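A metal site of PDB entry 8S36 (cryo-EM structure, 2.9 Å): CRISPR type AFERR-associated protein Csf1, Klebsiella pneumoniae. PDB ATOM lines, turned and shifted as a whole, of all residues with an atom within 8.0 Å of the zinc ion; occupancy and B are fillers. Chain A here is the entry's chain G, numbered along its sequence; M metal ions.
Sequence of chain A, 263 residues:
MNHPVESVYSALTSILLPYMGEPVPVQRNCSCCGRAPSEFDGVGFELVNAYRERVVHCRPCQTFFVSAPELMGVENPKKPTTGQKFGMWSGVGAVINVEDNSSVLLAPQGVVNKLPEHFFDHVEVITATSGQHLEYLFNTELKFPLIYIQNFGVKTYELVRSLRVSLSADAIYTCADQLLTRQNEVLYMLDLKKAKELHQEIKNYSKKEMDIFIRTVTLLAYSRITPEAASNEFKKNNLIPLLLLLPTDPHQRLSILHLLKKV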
ATOM      1  N   VAL A   5       7.339   0.356 -17.310  1.00  0.00           N
ATOM      2  CA  VAL A   5       6.618  -0.841 -17.720  1.00  0.00           C
ATOM      3  C   VAL A   5       6.389  -0.808 -19.217  1.00  0.00           C
ATOM      4  O   VAL A   5       6.433  -1.858 -19.879  1.00  0.00           O
ATOM      5  CB  VAL A   5       5.289  -0.981 -16.949  1.00  0.00           C
ATOM      6  CG1 VAL A   5       4.772  -2.409 -17.038  1.00  0.00           C
ATOM      7  CG2 VAL A   5       5.434  -0.568 -15.493  1.00  0.00           C
ATOM      8  N   GLU A   6       6.191   0.375 -19.792  1.00  0.00           N
ATOM      9  CA  GLU A   6       6.093   0.480 -21.242  1.00  0.00           C
ATOM     10  C   GLU A   6       7.409   0.102 -21.896  1.00  0.00           C
ATOM     11  O   GLU A   6       7.424  -0.527 -22.959  1.00  0.00           O
ATOM     12  CB  GLU A   6       5.696   1.898 -21.628  1.00  0.00           C
ATOM     13  CG  GLU A   6       4.236   2.216 -21.405  1.00  0.00           C
ATOM     14  CD  GLU A   6       3.900   2.432 -19.940  1.00  0.00           C
ATOM     15  OE1 GLU A   6       4.445   1.697 -19.092  1.00  0.00           O
ATOM     16  OE2 GLU A   6       3.083   3.331 -19.637  1.00  0.00           O
ATOM     17  N   ASN A  29      -8.134   3.566 -13.184  1.00  0.00           N
ATOM     18  CA  ASN A  29      -6.687   3.437 -13.296  1.00  0.00           C
ATOM     19  C   ASN A  29      -6.272   1.976 -13.155  1.00  0.00           C
ATOM     20  O   ASN A  29      -6.888   1.205 -12.411  1.00  0.00           O
ATOM     21  CB  ASN A  29      -5.989   4.277 -12.217  1.00  0.00           C
ATOM     22  CG  ASN A  29      -6.469   3.955 -10.825  1.00  0.00           C
ATOM     23  OD1 ASN A  29      -7.372   3.128 -10.631  1.00  0.00           O
ATOM     24  ND2 ASN A  29      -5.872   4.589  -9.821  1.00  0.00           N
ATOM     25  N   CYS A  30      -5.240   1.591 -13.901  1.00  0.00           N
ATOM     26  CA  CYS A  30      -4.777   0.209 -13.870  1.00  0.00           C
ATOM     27  C   CYS A  30      -4.366  -0.172 -12.457  1.00  0.00           C
ATOM     28  O   CYS A  30      -3.561   0.500 -11.815  1.00  0.00           O
ATOM     29  CB  CYS A  30      -3.586   0.033 -14.821  1.00  0.00           C
ATOM     30  SG  CYS A  30      -2.632  -1.471 -14.515  1.00  0.00           S
ATOM     31  N   SER A  31      -4.925  -1.284 -11.970  1.00  0.00           N
ATOM     32  CA  SER A  31      -4.658  -1.725 -10.606  1.00  0.00           C
ATOM     33  C   SER A  31      -3.262  -2.309 -10.444  1.00  0.00           C
ATOM     34  O   SER A  31      -2.801  -2.446  -9.303  1.00  0.00           O
ATOM     35  CB  SER A  31      -5.698  -2.760 -10.182  1.00  0.00           C
ATOM     36  OG  SER A  31      -5.247  -3.502  -9.061  1.00  0.00           O
ATOM     37  N   CYS A  32      -2.576  -2.636 -11.532  1.00  0.00           N
ATOM     38  CA  CYS A  32      -1.307  -3.353 -11.430  1.00  0.00           C
ATOM     39  C   CYS A  32      -0.130  -2.390 -11.294  1.00  0.00           C
ATOM     40  O   CYS A  32       0.627  -2.465 -10.324  1.00  0.00           O
ATOM     41  CB  CYS A  32      -1.144  -4.273 -12.646  1.00  0.00           C
ATOM     42  SG  CYS A  32       0.500  -4.984 -12.878  1.00  0.00           S
ATOM     43  N   CYS A  33       0.038  -1.486 -12.269  1.00  0.00           N
ATOM     44  CA  CYS A  33       1.010  -0.409 -12.101  1.00  0.00           C
ATOM     45  C   CYS A  33       0.500   0.663 -11.157  1.00  0.00           C
ATOM     46  O   CYS A  33       1.301   1.278 -10.429  1.00  0.00           O
ATOM     47  CB  CYS A  33       1.370   0.210 -13.445  1.00  0.00           C
ATOM     48  SG  CYS A  33      -0.010   0.985 -14.310  1.00  0.00           S
ATOM     49  N   GLY A  34      -0.811   0.906 -11.135  1.00  0.00           N
ATOM     50  CA  GLY A  34      -1.399   1.960 -10.336  1.00  0.00           C
ATOM     51  C   GLY A  34      -1.478   3.304 -11.012  1.00  0.00           C
ATOM     52  O   GLY A  34      -2.086   4.231 -10.448  1.00  0.00           O
ATOM     53  N   ARG A  35      -0.893   3.455 -12.202  1.00  0.00           N
ATOM     54  CA  ARG A  35      -0.894   4.746 -12.876  1.00  0.00           C
ATOM     55  C   ARG A  35      -2.284   5.068 -13.428  1.00  0.00           C
ATOM     56  O   ARG A  35      -3.087   4.181 -13.709  1.00  0.00           O
ATOM     57  CB  ARG A  35       0.132   4.767 -14.016  1.00  0.00           C
ATOM     58  CG  ARG A  35       1.489   4.141 -13.701  1.00  0.00           C
ATOM     59  CD  ARG A  35       2.248   3.773 -14.965  1.00  0.00           C
ATOM     60  NE  ARG A  35       1.552   2.750 -15.752  1.00  0.00           N
ATOM     61  CZ  ARG A  35       2.119   1.959 -16.642  1.00  0.00           C
ATOM     62  NH1 ARG A  35       3.416   2.007 -16.887  1.00  0.00           N
ATOM     63  NH2 ARG A  35       1.371   1.085 -17.304  1.00  0.00           N
ATOM     64  N   ALA A  36      -2.555   6.368 -13.590  1.00  0.00           N
ATOM     65  CA  ALA A  36      -3.858   6.797 -14.050  1.00  0.00           C
ATOM     66  C   ALA A  36      -4.057   6.450 -15.526  1.00  0.00           C
ATOM     67  O   ALA A  36      -3.086   6.272 -16.261  1.00  0.00           O
ATOM     68  CB  ALA A  36      -4.016   8.309 -13.849  1.00  0.00           C
ATOM     69  N   GLU A  39      -2.520   7.958 -19.688  1.00  0.00           N
ATOM     70  CA  GLU A  39      -1.526   7.510 -20.660  1.00  0.00           C
ATOM     71  C   GLU A  39      -1.894   6.202 -21.356  1.00  0.00           C
ATOM     72  O   GLU A  39      -1.192   5.806 -22.291  1.00  0.00           O
ATOM     73  CB  GLU A  39      -0.155   7.353 -19.981  1.00  0.00           C
ATOM     74  CG  GLU A  39      -0.138   6.426 -18.774  1.00  0.00           C
ATOM     75  CD  GLU A  39      -0.396   7.166 -17.476  1.00  0.00           C
ATOM     76  OE1 GLU A  39      -1.027   8.236 -17.511  1.00  0.00           O
ATOM     77  OE2 GLU A  39       0.037   6.668 -16.420  1.00  0.00           O
ATOM     78  N   PHE A  40      -2.954   5.527 -20.929  1.00  0.00           N
ATOM     79  CA  PHE A  40      -3.416   4.317 -21.591  1.00  0.00           C
ATOM     80  C   PHE A  40      -4.326   4.604 -22.773  1.00  0.00           C
ATOM     81  O   PHE A  40      -4.899   3.666 -23.342  1.00  0.00           O
ATOM     82  CB  PHE A  40      -4.120   3.395 -20.584  1.00  0.00           C
ATOM     83  CG  PHE A  40      -3.317   3.095 -19.346  1.00  0.00           C
ATOM     84  CD1 PHE A  40      -1.934   3.125 -19.359  1.00  0.00           C
ATOM     85  CD2 PHE A  40      -3.958   2.774 -18.158  1.00  0.00           C
ATOM     86  CE1 PHE A  40      -1.202   2.857 -18.227  1.00  0.00           C
ATOM     87  CE2 PHE A  40      -3.230   2.503 -17.014  1.00  0.00           C
ATOM     88  CZ  PHE A  40      -1.854   2.548 -17.041  1.00  0.00           C
ATOM     89  N   VAL A  56      -7.795  -4.308 -13.663  1.00  0.00           N
ATOM     90  CA  VAL A  56      -7.539  -3.682 -14.945  1.00  0.00           C
ATOM     91  C   VAL A  56      -6.034  -3.634 -15.146  1.00  0.00           C
ATOM     92  O   VAL A  56      -5.285  -3.234 -14.242  1.00  0.00           O
ATOM     93  CB  VAL A  56      -8.149  -2.280 -15.006  1.00  0.00           C
ATOM     94  CG1 VAL A  56      -8.078  -1.733 -16.428  1.00  0.00           C
ATOM     95  CG2 VAL A  56      -9.580  -2.303 -14.504  1.00  0.00           C
ATOM     96  N   HIS A  57      -5.581  -4.045 -16.332  1.00  0.00           N
ATOM     97  CA  HIS A  57      -4.183  -3.969 -16.717  1.00  0.00           C
ATOM     98  C   HIS A  57      -4.065  -3.111 -17.966  1.00  0.00           C
ATOM     99  O   HIS A  57      -4.939  -3.147 -18.830  1.00  0.00           O
ATOM    100  CB  HIS A  57      -3.599  -5.355 -16.975  1.00  0.00           C
ATOM    101  CG  HIS A  57      -3.588  -6.256 -15.779  1.00  0.00           C
ATOM    102  ND1 HIS A  57      -3.479  -5.764 -14.498  1.00  0.00           N
ATOM    103  CD2 HIS A  57      -3.661  -7.597 -15.670  1.00  0.00           C
ATOM    104  CE1 HIS A  57      -3.494  -6.779 -13.646  1.00  0.00           C
ATOM    105  NE2 HIS A  57      -3.605  -7.904 -14.334  1.00  0.00           N
ATOM    106  N   CYS A  58      -2.987  -2.348 -18.066  1.00  0.00           N
ATOM    107  CA  CYS A  58      -2.728  -1.611 -19.297  1.00  0.00           C
ATOM    108  C   CYS A  58      -2.009  -2.520 -20.289  1.00  0.00           C
ATOM    109  O   CYS A  58      -1.671  -3.662 -19.983  1.00  0.00           O
ATOM    110  CB  CYS A  58      -1.929  -0.348 -19.003  1.00  0.00           C
ATOM    111  SG  CYS A  58      -0.694  -0.534 -17.714  1.00  0.00           S
ATOM    112  N   ARG A  59      -1.784  -2.007 -21.493  1.00  0.00           N
ATOM    113  CA  ARG A  59      -1.100  -2.786 -22.514  1.00  0.00           C
ATOM    114  C   ARG A  59       0.234  -3.339 -22.010  1.00  0.00           C
ATOM    115  O   ARG A  59       0.503  -4.525 -22.258  1.00  0.00           O
ATOM    116  CB  ARG A  59      -0.911  -1.935 -23.775  1.00  0.00           C
ATOM    117  CG  ARG A  59      -0.456  -2.713 -25.004  1.00  0.00           C
ATOM    118  CD  ARG A  59      -1.615  -3.015 -25.938  1.00  0.00           C
ATOM    119  NE  ARG A  59      -2.219  -1.818 -26.508  1.00  0.00           N
ATOM    120  CZ  ARG A  59      -1.659  -1.041 -27.421  1.00  0.00           C
ATOM    121  NH1 ARG A  59      -0.450  -1.308 -27.903  1.00  0.00           N
ATOM    122  NH2 ARG A  59      -2.309   0.026 -27.854  1.00  0.00           N
ATOM    123  N   PRO A  60       1.084  -2.572 -21.319  1.00  0.00           N
ATOM    124  CA  PRO A  60       2.301  -3.182 -20.781  1.00  0.00           C
ATOM    125  C   PRO A  60       2.040  -4.127 -19.627  1.00  0.00           C
ATOM    126  O   PRO A  60       2.686  -5.184 -19.537  1.00  0.00           O
ATOM    127  CB  PRO A  60       3.136  -1.969 -20.337  1.00  0.00           C
ATOM    128  CG  PRO A  60       2.469  -0.778 -20.926  1.00  0.00           C
ATOM    129  CD  PRO A  60       1.032  -1.133 -21.031  1.00  0.00           C
ATOM    130  N   CYS A  61       1.109  -3.791 -18.736  1.00  0.00           N
ATOM    131  CA  CYS A  61       0.902  -4.610 -17.537  1.00  0.00           C
ATOM    132  C   CYS A  61       0.269  -5.946 -17.876  1.00  0.00           C
ATOM    133  O   CYS A  61       0.603  -6.968 -17.269  1.00  0.00           O
ATOM    134  CB  CYS A  61       0.035  -3.853 -16.532  1.00  0.00           C
ATOM    135  SG  CYS A  61       0.942  -2.751 -15.407  1.00  0.00           S
ATOM    136  N   GLN A  62      -0.655  -5.963 -18.849  1.00  0.00           N
ATOM    137  CA  GLN A  62      -1.364  -7.201 -19.164  1.00  0.00           C
ATOM    138  C   GLN A  62      -0.419  -8.265 -19.714  1.00  0.00           C
ATOM    139  O   GLN A  62      -0.694  -9.463 -19.564  1.00  0.00           O
ATOM    140  CB  GLN A  62      -2.478  -6.908 -20.167  1.00  0.00           C
ATOM    141  CG  GLN A  62      -3.162  -8.146 -20.737  1.00  0.00           C
ATOM    142  CD  GLN A  62      -3.699  -9.063 -19.654  1.00  0.00           C
ATOM    143  OE1 GLN A  62      -4.081  -8.607 -18.578  1.00  0.00           O
ATOM    144  NE2 GLN A  62      -3.735 -10.362 -19.942  1.00  0.00           N
ATOM    145  N   PHE A  64       2.217  -9.399 -18.631  1.00  0.00           N
ATOM    146  CA  PHE A  64       2.757 -10.283 -17.604  1.00  0.00           C
ATOM    147  C   PHE A  64       1.773 -11.372 -17.202  1.00  0.00           C
ATOM    148  O   PHE A  64       2.177 -12.350 -16.564  1.00  0.00           O
ATOM    149  CB  PHE A  64       3.143  -9.468 -16.367  1.00  0.00           C
ATOM    150  CG  PHE A  64       4.308  -8.553 -16.591  1.00  0.00           C
ATOM    151  CD1 PHE A  64       5.609  -9.017 -16.468  1.00  0.00           C
ATOM    152  CD2 PHE A  64       4.111  -7.221 -16.927  1.00  0.00           C
ATOM    153  CE1 PHE A  64       6.681  -8.178 -16.678  1.00  0.00           C
ATOM    154  CE2 PHE A  64       5.187  -6.385 -17.127  1.00  0.00           C
ATOM    155  CZ  PHE A  64       6.464  -6.855 -17.008  1.00  0.00           C
ATOM    156  N   PHE A  65       0.494 -11.240 -17.562  1.00  0.00           N
ATOM    157  CA  PHE A  65      -0.546 -12.187 -17.186  1.00  0.00           C
ATOM    158  C   PHE A  65      -1.069 -12.983 -18.387  1.00  0.00           C
ATOM    159  O   PHE A  65      -2.133 -13.585 -18.304  1.00  0.00           O
ATOM    160  CB  PHE A  65      -1.704 -11.461 -16.500  1.00  0.00           C
ATOM    161  CG  PHE A  65      -1.285 -10.647 -15.313  1.00  0.00           C
ATOM    162  CD1 PHE A  65      -0.817  -9.357 -15.472  1.00  0.00           C
ATOM    163  CD2 PHE A  65      -1.356 -11.172 -14.034  1.00  0.00           C
ATOM    164  CE1 PHE A  65      -0.434  -8.603 -14.384  1.00  0.00           C
ATOM    165  CE2 PHE A  65      -0.968 -10.420 -12.937  1.00  0.00           C
ATOM    166  CZ  PHE A  65      -0.509  -9.134 -13.116  1.00  0.00           C
ATOM    167  N   TYR A 157       2.509  -7.168  -9.360  1.00  0.00           N
ATOM    168  CA  TYR A 157       2.212  -5.795  -8.984  1.00  0.00           C
ATOM    169  C   TYR A 157       3.425  -5.111  -8.363  1.00  0.00           C
ATOM    170  O   TYR A 157       3.732  -3.951  -8.681  1.00  0.00           O
ATOM    171  CB  TYR A 157       1.028  -5.761  -8.018  1.00  0.00           C
ATOM    172  CG  TYR A 157      -0.215  -6.483  -8.535  1.00  0.00           C
ATOM    173  CD1 TYR A 157      -0.538  -6.463  -9.877  1.00  0.00           C
ATOM    174  CD2 TYR A 157      -1.047  -7.178  -7.663  1.00  0.00           C
ATOM    175  CE1 TYR A 157      -1.662  -7.109 -10.351  1.00  0.00           C
ATOM    176  CE2 TYR A 157      -2.180  -7.824  -8.133  1.00  0.00           C
ATOM    177  CZ  TYR A 157      -2.473  -7.785  -9.482  1.00  0.00           C
ATOM    178  OH  TYR A 157      -3.593  -8.434  -9.947  1.00  0.00           O
ATOM    179  N   VAL A 160       6.061  -4.450 -11.219  1.00  0.00           N
ATOM    180  CA  VAL A 160       5.802  -3.264 -12.021  1.00  0.00           C
ATOM    181  C   VAL A 160       6.030  -2.006 -11.199  1.00  0.00           C
ATOM    182  O   VAL A 160       6.622  -1.036 -11.684  1.00  0.00           O
ATOM    183  CB  VAL A 160       4.386  -3.312 -12.628  1.00  0.00           C
ATOM    184  CG1 VAL A 160       4.244  -4.510 -13.550  1.00  0.00           C
ATOM    185  CG2 VAL A 160       3.303  -3.323 -11.563  1.00  0.00           C
HETATM  186 ZN    ZN M   1      -0.559  -0.978 -15.442  1.00  0.00          ZN
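SG of Cys 58 is bound to the zinc ion, at 2.3 Å.
The zinc ion is bound by the side-chain sulfur (SG) of Cys 61 (2.3 Å).
The side-chain sulfur (SG) of Cys 30 binds the zinc ion (2.3 Å).
SG of Cys 33 is bound to the zinc ion, at 2.3 Å.
The side-chain sulfur (SG) of Cys 58 lies close to the guanidinium group (NH2) of Arg 35, 2.7 Å away.
The side-chain sulfur (SG) of Cys 32 sits close to the side-chain sulfur (SG) of Cys 61, 3.4 Å away.
The backbone NH (N) of Cys 30 lies within hydrogen-bond range of the backbone carbonyl oxygen (O) of Arg 35 (3.4 Å).
N of Cys 32 sits close to SG of Cys 30 (3.2 Å).
SG of Cys 30 sits close to O of Val 56, at 3.2 Å.
The side-chain sulfur of Cys 33 lies close to the guanidinium group of Arg 35, 2.8 Å away.
The guanidinium group (NH1) of Arg 35 lies within salt-bridge range of the side-chain carboxylate (OE1) of Glu 6.
Residues that only touch the zinc ion: Arg 35 (3.4 Å).
Along chain A the residues within 4 Å of the zinc ion span positions 30 to 61.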
